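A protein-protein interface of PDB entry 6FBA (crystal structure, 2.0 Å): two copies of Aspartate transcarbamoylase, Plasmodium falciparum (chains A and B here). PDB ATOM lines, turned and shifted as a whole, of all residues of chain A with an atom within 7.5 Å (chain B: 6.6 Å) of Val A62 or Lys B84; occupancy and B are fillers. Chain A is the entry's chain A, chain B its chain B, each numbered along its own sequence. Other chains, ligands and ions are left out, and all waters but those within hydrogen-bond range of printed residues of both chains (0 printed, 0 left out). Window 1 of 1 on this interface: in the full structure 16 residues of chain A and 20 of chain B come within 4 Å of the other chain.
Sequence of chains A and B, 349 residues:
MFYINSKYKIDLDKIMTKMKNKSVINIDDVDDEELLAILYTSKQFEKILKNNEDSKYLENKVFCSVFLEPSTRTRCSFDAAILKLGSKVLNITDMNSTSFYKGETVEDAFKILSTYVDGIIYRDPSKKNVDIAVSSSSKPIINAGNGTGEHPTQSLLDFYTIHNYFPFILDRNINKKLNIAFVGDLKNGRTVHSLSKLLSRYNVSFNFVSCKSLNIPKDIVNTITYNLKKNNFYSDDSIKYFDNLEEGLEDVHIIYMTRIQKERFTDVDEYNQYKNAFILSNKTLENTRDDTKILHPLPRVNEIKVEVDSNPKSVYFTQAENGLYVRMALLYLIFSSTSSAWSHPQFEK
O of Ser B87 is in hydrogen-bond range of NZ of Lys A88, at 3.0 Å.
Of the 18 printed residues of chain A, 7 touch a printed residue of chain B.
Printed residues of chain A that touch a printed residue of chain B: Glu A59, Asn A60, Val A62, Lys A88, Leu A90, Thr A115 and Tyr A116.
Among the printed residues, no Asp or Glu carboxylate lies within 4 Å of a Lys or Arg side-chain nitrogen of the other chain.
Printed residues of chain B within 4 Å of Val A62: Lys B84 (3.8 Å).
Printed residues of chain A within 4 Å of Lys B84: Val A62.
Of the printed residues of chain B, Thr A115 touches Leu B324.
Of the printed residues of chain B, Tyr A116 touches Ala B80 (3.9 Å) and Leu B324 (3.9 Å).
Of the printed residues of chain A, Ser B87 touches Lys A88.
Printed residues of chain B within 4 Å of Glu A59: Lys B56.
Of the printed residues of chain B, Lys A88 touches Leu B83, Gly B86 and Ser B87.
2 positions are printed for both chains.
Glu A59 touches Lys B56 (O to NZ, 3.9 Å).
Lys B56 touches Asn A60.
Lys B84 touches Val A62.
Lys A88 touches Leu B83 (CD to O, 3.6 Å).
NZ of Lys A88 touches O of Gly B86, 3.7 Å away.
CD2 of Leu A90 touches CA of Ala B80, 3.97 Å away.
Leu B324 touches Thr A115 (CD2 to O, 3.8 Å).
Ala B80 touches Tyr A116 (CB to O, 3.9 Å).
Tyr A116 touches Leu B324 (CD1 to CB, 3.9 Å).
N of Val A62 lies within hydrogen-bond range of OD2 of Asp A118.
O of Leu A90 sits close to SG of Cys A64 (3.7 Å).
The backbone carbonyl oxygen (O) of Phe A63 sits at hydrogen-bond distance from the backbone NH (N) of Leu A90, at 3.0 Å.
The backbone carbonyl oxygen (O) of Lys A61 sits at hydrogen-bond distance from the backbone NH (N) of Lys A88.
The backbone carbonyl oxygen (O) of Ile B82 lies within hydrogen-bond range of the backbone NH (N) of Ser B87, at 3.2 Å.
The side-chain hydroxyl (OG) of Ser B55 sits at hydrogen-bond distance from the side-chain amino group (NZ) of Lys B84.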
ATOM      1  N   GLU A  59      -1.530  25.098 -20.185  1.00  0.00           N
ATOM      2  CA  GLU A  59      -1.925  23.846 -19.523  1.00  0.00           C
ATOM      3  C   GLU A  59      -1.643  22.469 -20.063  1.00  0.00           C
ATOM      4  O   GLU A  59      -1.618  21.523 -19.272  1.00  0.00           O
ATOM      5  CB  GLU A  59      -3.424  23.838 -19.312  1.00  0.00           C
ATOM      6  CG  GLU A  59      -3.855  24.734 -18.215  1.00  0.00           C
ATOM      7  CD  GLU A  59      -5.289  24.479 -17.813  1.00  0.00           C
ATOM      8  OE1 GLU A  59      -6.087  25.343 -18.205  1.00  0.00           O
ATOM      9  OE2 GLU A  59      -5.605  23.416 -17.161  1.00  0.00           O
ATOM     10  N   ASN A  60      -1.512  22.273 -21.335  1.00  0.00           N
ATOM     11  CA  ASN A  60      -1.512  20.888 -21.796  1.00  0.00           C
ATOM     12  C   ASN A  60      -0.163  20.368 -22.265  1.00  0.00           C
ATOM     13  O   ASN A  60      -0.104  19.489 -23.022  1.00  0.00           O
ATOM     14  CB  ASN A  60      -2.549  20.794 -22.884  1.00  0.00           C
ATOM     15  CG  ASN A  60      -3.943  21.112 -22.347  1.00  0.00           C
ATOM     16  OD1 ASN A  60      -4.439  20.534 -21.349  1.00  0.00           O
ATOM     17  ND2 ASN A  60      -4.569  22.075 -22.987  1.00  0.00           N
ATOM     18  N   LYS A  61       0.917  20.879 -21.706  1.00  0.00           N
ATOM     19  CA  LYS A  61       2.177  20.530 -22.143  1.00  0.00           C
ATOM     20  C   LYS A  61       2.829  19.616 -21.142  1.00  0.00           C
ATOM     21  O   LYS A  61       2.533  19.674 -19.920  1.00  0.00           O
ATOM     22  CB  LYS A  61       3.026  21.814 -22.341  1.00  0.00           C
ATOM     23  CG  LYS A  61       2.701  22.752 -23.489  1.00  0.00           C
ATOM     24  CD  LYS A  61       2.034  22.130 -24.708  1.00  0.00           C
ATOM     25  CE  LYS A  61       1.374  23.242 -25.507  1.00  0.00           C
ATOM     26  NZ  LYS A  61       1.629  22.819 -26.881  1.00  0.00           N
ATOM     27  N   VAL A  62       3.734  18.778 -21.650  1.00  0.00           N
ATOM     28  CA  VAL A  62       4.581  17.922 -20.826  1.00  0.00           C
ATOM     29  C   VAL A  62       6.024  18.218 -21.176  1.00  0.00           C
ATOM     30  O   VAL A  62       6.425  18.051 -22.318  1.00  0.00           O
ATOM     31  CB  VAL A  62       4.278  16.453 -21.021  1.00  0.00           C
ATOM     32  CG1 VAL A  62       5.081  15.560 -20.099  1.00  0.00           C
ATOM     33  CG2 VAL A  62       2.814  16.154 -20.850  1.00  0.00           C
ATOM     34  N   PHE A  63       6.826  18.574 -20.153  1.00  0.00           N
ATOM     35  CA  PHE A  63       8.218  18.865 -20.314  1.00  0.00           C
ATOM     36  C   PHE A  63       9.127  17.833 -19.707  1.00  0.00           C
ATOM     37  O   PHE A  63       8.728  17.109 -18.817  1.00  0.00           O
ATOM     38  CB  PHE A  63       8.595  20.241 -19.753  1.00  0.00           C
ATOM     39  CG  PHE A  63       7.831  21.391 -20.393  1.00  0.00           C
ATOM     40  CD1 PHE A  63       6.632  21.829 -19.924  1.00  0.00           C
ATOM     41  CD2 PHE A  63       8.366  22.038 -21.465  1.00  0.00           C
ATOM     42  CE1 PHE A  63       5.927  22.850 -20.520  1.00  0.00           C
ATOM     43  CE2 PHE A  63       7.654  23.041 -22.128  1.00  0.00           C
ATOM     44  CZ  PHE A  63       6.462  23.494 -21.589  1.00  0.00           C
ATOM     45  N   CYS A  64      10.374  17.776 -20.190  1.00  0.00           N
ATOM     46  CA  CYS A  64      11.375  17.008 -19.520  1.00  0.00           C
ATOM     47  C   CYS A  64      12.475  18.023 -19.055  1.00  0.00           C
ATOM     48  O   CYS A  64      12.935  18.789 -19.832  1.00  0.00           O
ATOM     49  CB  CYS A  64      11.975  15.881 -20.337  1.00  0.00           C
ATOM     50  SG  CYS A  64      13.167  14.937 -19.378  1.00  0.00           S
ATOM     51  N   ILE A  82       7.012  25.858 -14.701  1.00  0.00           N
ATOM     52  CA  ILE A  82       6.213  24.893 -15.457  1.00  0.00           C
ATOM     53  C   ILE A  82       4.876  24.554 -14.769  1.00  0.00           C
ATOM     54  O   ILE A  82       3.795  24.547 -15.387  1.00  0.00           O
ATOM     55  CB  ILE A  82       7.027  23.601 -15.745  1.00  0.00           C
ATOM     56  CG1 ILE A  82       8.194  23.937 -16.676  1.00  0.00           C
ATOM     57  CG2 ILE A  82       6.151  22.501 -16.381  1.00  0.00           C
ATOM     58  CD1 ILE A  82       9.241  22.841 -16.542  1.00  0.00           C
ATOM     59  N   SER A  87       1.288  23.209 -16.612  1.00  0.00           N
ATOM     60  CA  SER A  87       1.897  22.078 -17.328  1.00  0.00           C
ATOM     61  C   SER A  87       2.524  21.045 -16.399  1.00  0.00           C
ATOM     62  O   SER A  87       2.421  21.155 -15.154  1.00  0.00           O
ATOM     63  CB  SER A  87       2.831  22.682 -18.429  1.00  0.00           C
ATOM     64  OG  SER A  87       1.879  23.032 -19.495  1.00  0.00           O
ATOM     65  N   LYS A  88       3.111  19.996 -16.969  1.00  0.00           N
ATOM     66  CA  LYS A  88       3.672  18.873 -16.231  1.00  0.00           C
ATOM     67  C   LYS A  88       5.143  18.702 -16.638  1.00  0.00           C
ATOM     68  O   LYS A  88       5.568  19.130 -17.680  1.00  0.00           O
ATOM     69  CB  LYS A  88       2.848  17.572 -16.411  1.00  0.00           C
ATOM     70  CG  LYS A  88       1.432  17.683 -16.028  1.00  0.00           C
ATOM     71  CD  LYS A  88       0.671  16.404 -16.468  1.00  0.00           C
ATOM     72  CE  LYS A  88      -0.805  16.475 -16.174  1.00  0.00           C
ATOM     73  NZ  LYS A  88      -1.096  16.116 -14.743  1.00  0.00           N
ATOM     74  N   VAL A  89       5.907  18.067 -15.768  1.00  0.00           N
ATOM     75  CA  VAL A  89       7.286  17.849 -15.935  1.00  0.00           C
ATOM     76  C   VAL A  89       7.776  16.552 -15.337  1.00  0.00           C
ATOM     77  O   VAL A  89       7.350  16.119 -14.265  1.00  0.00           O
ATOM     78  CB  VAL A  89       8.142  19.070 -15.414  1.00  0.00           C
ATOM     79  CG1 VAL A  89       8.063  19.287 -13.983  1.00  0.00           C
ATOM     80  CG2 VAL A  89       9.630  18.935 -15.812  1.00  0.00           C
ATOM     81  N   LEU A  90       8.657  15.902 -16.077  1.00  0.00           N
ATOM     82  CA  LEU A  90       9.436  14.803 -15.557  1.00  0.00           C
ATOM     83  C   LEU A  90      10.891  15.196 -15.529  1.00  0.00           C
ATOM     84  O   LEU A  90      11.358  15.988 -16.360  1.00  0.00           O
ATOM     85  CB  LEU A  90       9.238  13.534 -16.399  1.00  0.00           C
ATOM     86  CG  LEU A  90       9.555  13.580 -17.877  1.00  0.00           C
ATOM     87  CD1 LEU A  90      10.511  12.488 -18.288  1.00  0.00           C
ATOM     88  CD2 LEU A  90       8.330  13.382 -18.720  1.00  0.00           C
ATOM     89  N   THR A 115      10.803  12.746 -28.805  1.00  0.00           N
ATOM     90  CA  THR A 115       9.488  12.145 -29.204  1.00  0.00           C
ATOM     91  C   THR A 115       8.541  11.911 -28.035  1.00  0.00           C
ATOM     92  O   THR A 115       7.403  11.662 -28.197  1.00  0.00           O
ATOM     93  CB  THR A 115       9.667  10.860 -30.021  1.00  0.00           C
ATOM     94  OG1 THR A 115      10.189   9.814 -29.201  1.00  0.00           O
ATOM     95  CG2 THR A 115      10.622  11.146 -31.237  1.00  0.00           C
ATOM     96  N   TYR A 116       8.987  12.047 -26.801  1.00  0.00           N
ATOM     97  CA  TYR A 116       8.120  11.778 -25.633  1.00  0.00           C
ATOM     98  C   TYR A 116       7.526  13.042 -25.035  1.00  0.00           C
ATOM     99  O   TYR A 116       6.530  12.919 -24.354  1.00  0.00           O
ATOM    100  CB  TYR A 116       8.864  11.081 -24.513  1.00  0.00           C
ATOM    101  CG  TYR A 116       9.335   9.724 -24.797  1.00  0.00           C
ATOM    102  CD1 TYR A 116       8.740   8.949 -25.776  1.00  0.00           C
ATOM    103  CD2 TYR A 116      10.317   9.141 -23.998  1.00  0.00           C
ATOM    104  CE1 TYR A 116       9.125   7.649 -26.024  1.00  0.00           C
ATOM    105  CE2 TYR A 116      10.719   7.793 -24.258  1.00  0.00           C
ATOM    106  CZ  TYR A 116      10.102   7.095 -25.263  1.00  0.00           C
ATOM    107  OH  TYR A 116      10.468   5.829 -25.553  1.00  0.00           O
ATOM    108  N   VAL A 117       8.137  14.195 -25.242  1.00  0.00           N
ATOM    109  CA  VAL A 117       7.736  15.430 -24.554  1.00  0.00           C
ATOM    110  C   VAL A 117       7.613  16.598 -25.565  1.00  0.00           C
ATOM    111  O   VAL A 117       8.025  16.497 -26.700  1.00  0.00           O
ATOM    112  CB  VAL A 117       8.738  15.777 -23.413  1.00  0.00           C
ATOM    113  CG1 VAL A 117       8.801  14.647 -22.357  1.00  0.00           C
ATOM    114  CG2 VAL A 117      10.158  16.063 -23.970  1.00  0.00           C
ATOM    115  N   ASP A 118       7.043  17.703 -25.087  1.00  0.00           N
ATOM    116  CA  ASP A 118       6.810  18.919 -25.847  1.00  0.00           C
ATOM    117  C   ASP A 118       8.006  19.807 -25.815  1.00  0.00           C
ATOM    118  O   ASP A 118       8.174  20.599 -26.692  1.00  0.00           O
ATOM    119  CB  ASP A 118       5.601  19.656 -25.280  1.00  0.00           C
ATOM    120  CG  ASP A 118       4.326  18.838 -25.417  1.00  0.00           C
ATOM    121  OD1 ASP A 118       3.992  18.515 -26.556  1.00  0.00           O
ATOM    122  OD2 ASP A 118       3.611  18.562 -24.440  1.00  0.00           O
ATOM    123  N   GLY A 119       8.821  19.717 -24.777  1.00  0.00           N
ATOM    124  CA  GLY A 119      10.042  20.541 -24.806  1.00  0.00           C
ATOM    125  C   GLY A 119      10.897  20.100 -23.692  1.00  0.00           C
ATOM    126  O   GLY A 119      10.445  19.307 -22.848  1.00  0.00           O
ATOM    127  N   ILE A 120      12.152  20.551 -23.696  1.00  0.00           N
ATOM    128  CA  ILE A 120      13.164  20.036 -22.810  1.00  0.00           C
ATOM    129  C   ILE A 120      13.933  21.215 -22.211  1.00  0.00           C
ATOM    130  O   ILE A 120      14.392  22.117 -22.965  1.00  0.00           O
ATOM    131  CB  ILE A 120      14.125  19.086 -23.525  1.00  0.00           C
ATOM    132  CG1 ILE A 120      13.350  17.880 -24.116  1.00  0.00           C
ATOM    133  CG2 ILE A 120      15.231  18.593 -22.586  1.00  0.00           C
ATOM    134  CD1 ILE A 120      14.017  17.163 -25.325  1.00  0.00           C
ATOM    135  N   PHE A 335       5.903  27.956 -26.087  1.00  0.00           N
ATOM    136  CA  PHE A 335       5.092  26.780 -26.161  1.00  0.00           C
ATOM    137  C   PHE A 335       3.611  26.943 -26.317  1.00  0.00           C
ATOM    138  O   PHE A 335       2.935  25.917 -26.530  1.00  0.00           O
ATOM    139  CB  PHE A 335       5.411  25.874 -24.994  1.00  0.00           C
ATOM    140  CG  PHE A 335       6.831  25.360 -24.988  1.00  0.00           C
ATOM    141  CD1 PHE A 335       7.216  24.331 -25.800  1.00  0.00           C
ATOM    142  CD2 PHE A 335       7.792  25.962 -24.213  1.00  0.00           C
ATOM    143  CE1 PHE A 335       8.523  23.874 -25.819  1.00  0.00           C
ATOM    144  CE2 PHE A 335       9.110  25.481 -24.237  1.00  0.00           C
ATOM    145  CZ  PHE A 335       9.451  24.425 -25.012  1.00  0.00           C
ATOM    146  N   ILE B  48      -3.974  10.398 -32.343  1.00  0.00           N
ATOM    147  CA  ILE B  48      -4.231  11.559 -31.506  1.00  0.00           C
ATOM    148  C   ILE B  48      -2.962  12.446 -31.312  1.00  0.00           C
ATOM    149  O   ILE B  48      -2.976  13.621 -31.539  1.00  0.00           O
ATOM    150  CB  ILE B  48      -4.828  11.092 -30.166  1.00  0.00           C
ATOM    151  CG1 ILE B  48      -6.307  10.658 -30.399  1.00  0.00           C
ATOM    152  CG2 ILE B  48      -4.761  12.200 -29.122  1.00  0.00           C
ATOM    153  CD1 ILE B  48      -6.876   9.761 -29.330  1.00  0.00           C
ATOM    154  N   LEU B  49      -1.850  11.845 -30.955  1.00  0.00           N
ATOM    155  CA  LEU B  49      -0.625  12.590 -30.720  1.00  0.00           C
ATOM    156  C   LEU B  49      -0.097  13.195 -31.998  1.00  0.00           C
ATOM    157  O   LEU B  49       0.213  14.394 -32.015  1.00  0.00           O
ATOM    158  CB  LEU B  49       0.413  11.732 -30.029  1.00  0.00           C
ATOM    159  CG  LEU B  49       0.337  11.829 -28.482  1.00  0.00           C
ATOM    160  CD1 LEU B  49      -1.062  11.616 -27.988  1.00  0.00           C
ATOM    161  CD2 LEU B  49       1.275  10.866 -27.731  1.00  0.00           C
ATOM    162  N   GLU B  53      -3.872  16.425 -30.993  1.00  0.00           N
ATOM    163  CA  GLU B  53      -5.176  16.450 -30.346  1.00  0.00           C
ATOM    164  C   GLU B  53      -5.049  16.260 -28.835  1.00  0.00           C
ATOM    165  O   GLU B  53      -3.996  15.809 -28.333  1.00  0.00           O
ATOM    166  CB  GLU B  53      -6.104  15.427 -31.003  1.00  0.00           C
ATOM    167  CG  GLU B  53      -6.336  15.742 -32.509  1.00  0.00           C
ATOM    168  CD  GLU B  53      -7.136  14.654 -33.252  1.00  0.00           C
ATOM    169  OE1 GLU B  53      -7.352  14.703 -34.495  1.00  0.00           O
ATOM    170  OE2 GLU B  53      -7.527  13.687 -32.599  1.00  0.00           O
ATOM    171  N   ASP B  54      -6.111  16.613 -28.119  1.00  0.00           N
ATOM    172  CA  ASP B  54      -6.216  16.351 -26.705  1.00  0.00           C
ATOM    173  C   ASP B  54      -6.053  14.835 -26.384  1.00  0.00           C
ATOM    174  O   ASP B  54      -6.770  14.020 -26.890  1.00  0.00           O
ATOM    175  CB  ASP B  54      -7.547  16.870 -26.137  1.00  0.00           C
ATOM    176  CG  ASP B  54      -7.759  16.433 -24.577  1.00  0.00           C
ATOM    177  OD1 ASP B  54      -6.871  16.786 -23.811  1.00  0.00           O
ATOM    178  OD2 ASP B  54      -8.683  15.662 -24.109  1.00  0.00           O
ATOM    179  N   SER B  55      -5.109  14.481 -25.511  1.00  0.00           N
ATOM    180  CA  SER B  55      -4.864  13.099 -25.135  1.00  0.00           C
ATOM    181  C   SER B  55      -5.209  12.810 -23.641  1.00  0.00           C
ATOM    182  O   SER B  55      -4.792  11.814 -23.121  1.00  0.00           O
ATOM    183  CB  SER B  55      -3.412  12.702 -25.367  1.00  0.00           C
ATOM    184  OG  SER B  55      -2.539  13.504 -24.616  1.00  0.00           O
ATOM    185  N   LYS B  56      -5.975  13.651 -22.972  1.00  0.00           N
ATOM    186  CA  LYS B  56      -6.153  13.503 -21.526  1.00  0.00           C
ATOM    187  C   LYS B  56      -7.270  12.496 -21.228  1.00  0.00           C
ATOM    188  O   LYS B  56      -8.327  12.855 -20.842  1.00  0.00           O
ATOM    189  CB  LYS B  56      -6.367  14.862 -20.844  1.00  0.00           C
ATOM    190  CG  LYS B  56      -5.121  15.751 -20.843  1.00  0.00           C
ATOM    191  CD  LYS B  56      -5.364  16.984 -19.911  1.00  0.00           C
ATOM    192  CE  LYS B  56      -4.028  17.382 -19.251  1.00  0.00           C
ATOM    193  NZ  LYS B  56      -4.025  18.569 -18.315  1.00  0.00           N
ATOM    194  N   TYR B  57      -6.988  11.217 -21.393  1.00  0.00           N
ATOM    195  CA  TYR B  57      -8.028  10.184 -21.333  1.00  0.00           C
ATOM    196  C   TYR B  57      -8.008   9.536 -20.006  1.00  0.00           C
ATOM    197  O   TYR B  57      -8.763   8.644 -19.779  1.00  0.00           O
ATOM    198  CB  TYR B  57      -7.882   9.151 -22.436  1.00  0.00           C
ATOM    199  CG  TYR B  57      -8.469   9.641 -23.677  1.00  0.00           C
ATOM    200  CD1 TYR B  57      -7.719  10.453 -24.531  1.00  0.00           C
ATOM    201  CD2 TYR B  57      -9.794   9.417 -23.982  1.00  0.00           C
ATOM    202  CE1 TYR B  57      -8.248  10.956 -25.662  1.00  0.00           C
ATOM    203  CE2 TYR B  57     -10.335   9.937 -25.149  1.00  0.00           C
ATOM    204  CZ  TYR B  57      -9.524  10.684 -25.972  1.00  0.00           C
ATOM    205  OH  TYR B  57      -9.966  11.281 -27.120  1.00  0.00           O
ATOM    206  N   ASP B  79       6.723   7.712 -17.171  1.00  0.00           N
ATOM    207  CA  ASP B  79       6.227   8.988 -16.636  1.00  0.00           C
ATOM    208  C   ASP B  79       5.609   9.832 -17.756  1.00  0.00           C
ATOM    209  O   ASP B  79       4.578  10.422 -17.572  1.00  0.00           O
ATOM    210  CB  ASP B  79       7.312   9.865 -15.956  1.00  0.00           C
ATOM    211  CG  ASP B  79       7.886   9.326 -14.588  1.00  0.00           C
ATOM    212  OD1 ASP B  79       7.340   8.448 -13.944  1.00  0.00           O
ATOM    213  OD2 ASP B  79       9.028   9.815 -14.220  1.00  0.00           O
ATOM    214  N   ALA B  80       6.261   9.885 -18.923  1.00  0.00           N
ATOM    215  CA  ALA B  80       5.767  10.675 -20.079  1.00  0.00           C
ATOM    216  C   ALA B  80       4.369  10.208 -20.457  1.00  0.00           C
ATOM    217  O   ALA B  80       3.478  11.053 -20.700  1.00  0.00           O
ATOM    218  CB  ALA B  80       6.716  10.549 -21.240  1.00  0.00           C
ATOM    219  N   ALA B  81       4.155   8.882 -20.504  1.00  0.00           N
ATOM    220  CA  ALA B  81       2.858   8.357 -20.840  1.00  0.00           C
ATOM    221  C   ALA B  81       1.817   8.652 -19.776  1.00  0.00           C
ATOM    222  O   ALA B  81       0.677   9.024 -20.074  1.00  0.00           O
ATOM    223  CB  ALA B  81       2.965   6.838 -21.059  1.00  0.00           C
ATOM    224  N   ILE B  82       2.176   8.566 -18.501  1.00  0.00           N
ATOM    225  CA  ILE B  82       1.182   8.916 -17.459  1.00  0.00           C
ATOM    226  C   ILE B  82       0.740  10.363 -17.584  1.00  0.00           C
ATOM    227  O   ILE B  82      -0.459  10.705 -17.540  1.00  0.00           O
ATOM    228  CB  ILE B  82       1.786   8.638 -16.046  1.00  0.00           C
ATOM    229  CG1 ILE B  82       1.974   7.166 -15.795  1.00  0.00           C
ATOM    230  CG2 ILE B  82       0.949   9.239 -14.901  1.00  0.00           C
ATOM    231  CD1 ILE B  82       2.990   6.851 -14.686  1.00  0.00           C
ATOM    232  N   LEU B  83       1.758  11.251 -17.688  1.00  0.00           N
ATOM    233  CA  LEU B  83       1.493  12.681 -17.756  1.00  0.00           C
ATOM    234  C   LEU B  83       0.790  13.092 -19.034  1.00  0.00           C
ATOM    235  O   LEU B  83      -0.064  14.003 -19.045  1.00  0.00           O
ATOM    236  CB  LEU B  83       2.772  13.473 -17.556  1.00  0.00           C
ATOM    237  CG  LEU B  83       3.598  13.135 -16.288  1.00  0.00           C
ATOM    238  CD1 LEU B  83       5.014  13.662 -16.424  1.00  0.00           C
ATOM    239  CD2 LEU B  83       2.876  13.708 -15.018  1.00  0.00           C
ATOM    240  N   LYS B  84       1.144  12.465 -20.144  1.00  0.00           N
ATOM    241  CA  LYS B  84       0.380  12.738 -21.391  1.00  0.00           C
ATOM    242  C   LYS B  84      -1.093  12.363 -21.307  1.00  0.00           C
ATOM    243  O   LYS B  84      -1.956  13.026 -21.938  1.00  0.00           O
ATOM    244  CB  LYS B  84       1.005  12.026 -22.611  1.00  0.00           C
ATOM    245  CG  LYS B  84       2.140  12.813 -23.176  1.00  0.00           C
ATOM    246  CD  LYS B  84       1.656  14.093 -23.860  1.00  0.00           C
ATOM    247  CE  LYS B  84       0.756  13.925 -25.099  1.00  0.00           C
ATOM    248  NZ  LYS B  84      -0.322  15.003 -25.366  1.00  0.00           N
ATOM    249  N   LEU B  85      -1.389  11.322 -20.524  1.00  0.00           N
ATOM    250  CA  LEU B  85      -2.776  10.940 -20.291  1.00  0.00           C
ATOM    251  C   LEU B  85      -3.541  11.916 -19.355  1.00  0.00           C
ATOM    252  O   LEU B  85      -4.739  11.786 -19.205  1.00  0.00           O
ATOM    253  CB  LEU B  85      -2.846   9.506 -19.780  1.00  0.00           C
ATOM    254  CG  LEU B  85      -2.555   8.415 -20.842  1.00  0.00           C
ATOM    255  CD1 LEU B  85      -2.330   7.063 -20.229  1.00  0.00           C
ATOM    256  CD2 LEU B  85      -3.750   8.228 -21.803  1.00  0.00           C
ATOM    257  N   GLY B  86      -2.825  12.891 -18.715  1.00  0.00           N
ATOM    258  CA  GLY B  86      -3.448  13.887 -17.832  1.00  0.00           C
ATOM    259  C   GLY B  86      -3.424  13.443 -16.368  1.00  0.00           C
ATOM    260  O   GLY B  86      -4.006  14.049 -15.533  1.00  0.00           O
ATOM    261  N   SER B  87      -2.797  12.350 -16.090  1.00  0.00           N
ATOM    262  CA  SER B  87      -2.636  11.834 -14.782  1.00  0.00           C
ATOM    263  C   SER B  87      -1.342  12.385 -14.083  1.00  0.00           C
ATOM    264  O   SER B  87      -0.578  13.170 -14.699  1.00  0.00           O
ATOM    265  CB  SER B  87      -2.667  10.266 -14.850  1.00  0.00           C
ATOM    266  OG  SER B  87      -4.122  10.004 -14.794  1.00  0.00           O
ATOM    267  N   LEU B 324       5.745   5.227 -26.428  1.00  0.00           N
ATOM    268  CA  LEU B 324       4.864   6.219 -25.772  1.00  0.00           C
ATOM    269  C   LEU B 324       3.415   5.774 -25.977  1.00  0.00           C
ATOM    270  O   LEU B 324       2.642   5.673 -24.982  1.00  0.00           O
ATOM    271  CB  LEU B 324       5.095   7.619 -26.272  1.00  0.00           C
ATOM    272  CG  LEU B 324       4.147   8.726 -25.770  1.00  0.00           C
ATOM    273  CD1 LEU B 324       4.317   8.945 -24.290  1.00  0.00           C
ATOM    274  CD2 LEU B 324       4.401  10.021 -26.501  1.00  0.00           C
ATOM    275  N   MET B 328       0.777   4.407 -23.061  1.00  0.00           N
ATOM    276  CA  MET B 328      -0.496   5.114 -22.929  1.00  0.00           C
ATOM    277  C   MET B 328      -1.648   4.204 -23.055  1.00  0.00           C
ATOM    278  O   MET B 328      -2.573   4.235 -22.243  1.00  0.00           O
ATOM    279  CB  MET B 328      -0.560   6.278 -23.923  1.00  0.00           C
ATOM    280  CG  MET B 328       0.417   7.401 -23.594  1.00  0.00           C
ATOM    281  SD  MET B 328       0.380   8.761 -24.778  1.00  0.00           S
ATOM    282  CE  MET B 328      -1.137   9.603 -24.321  1.00  0.00           C
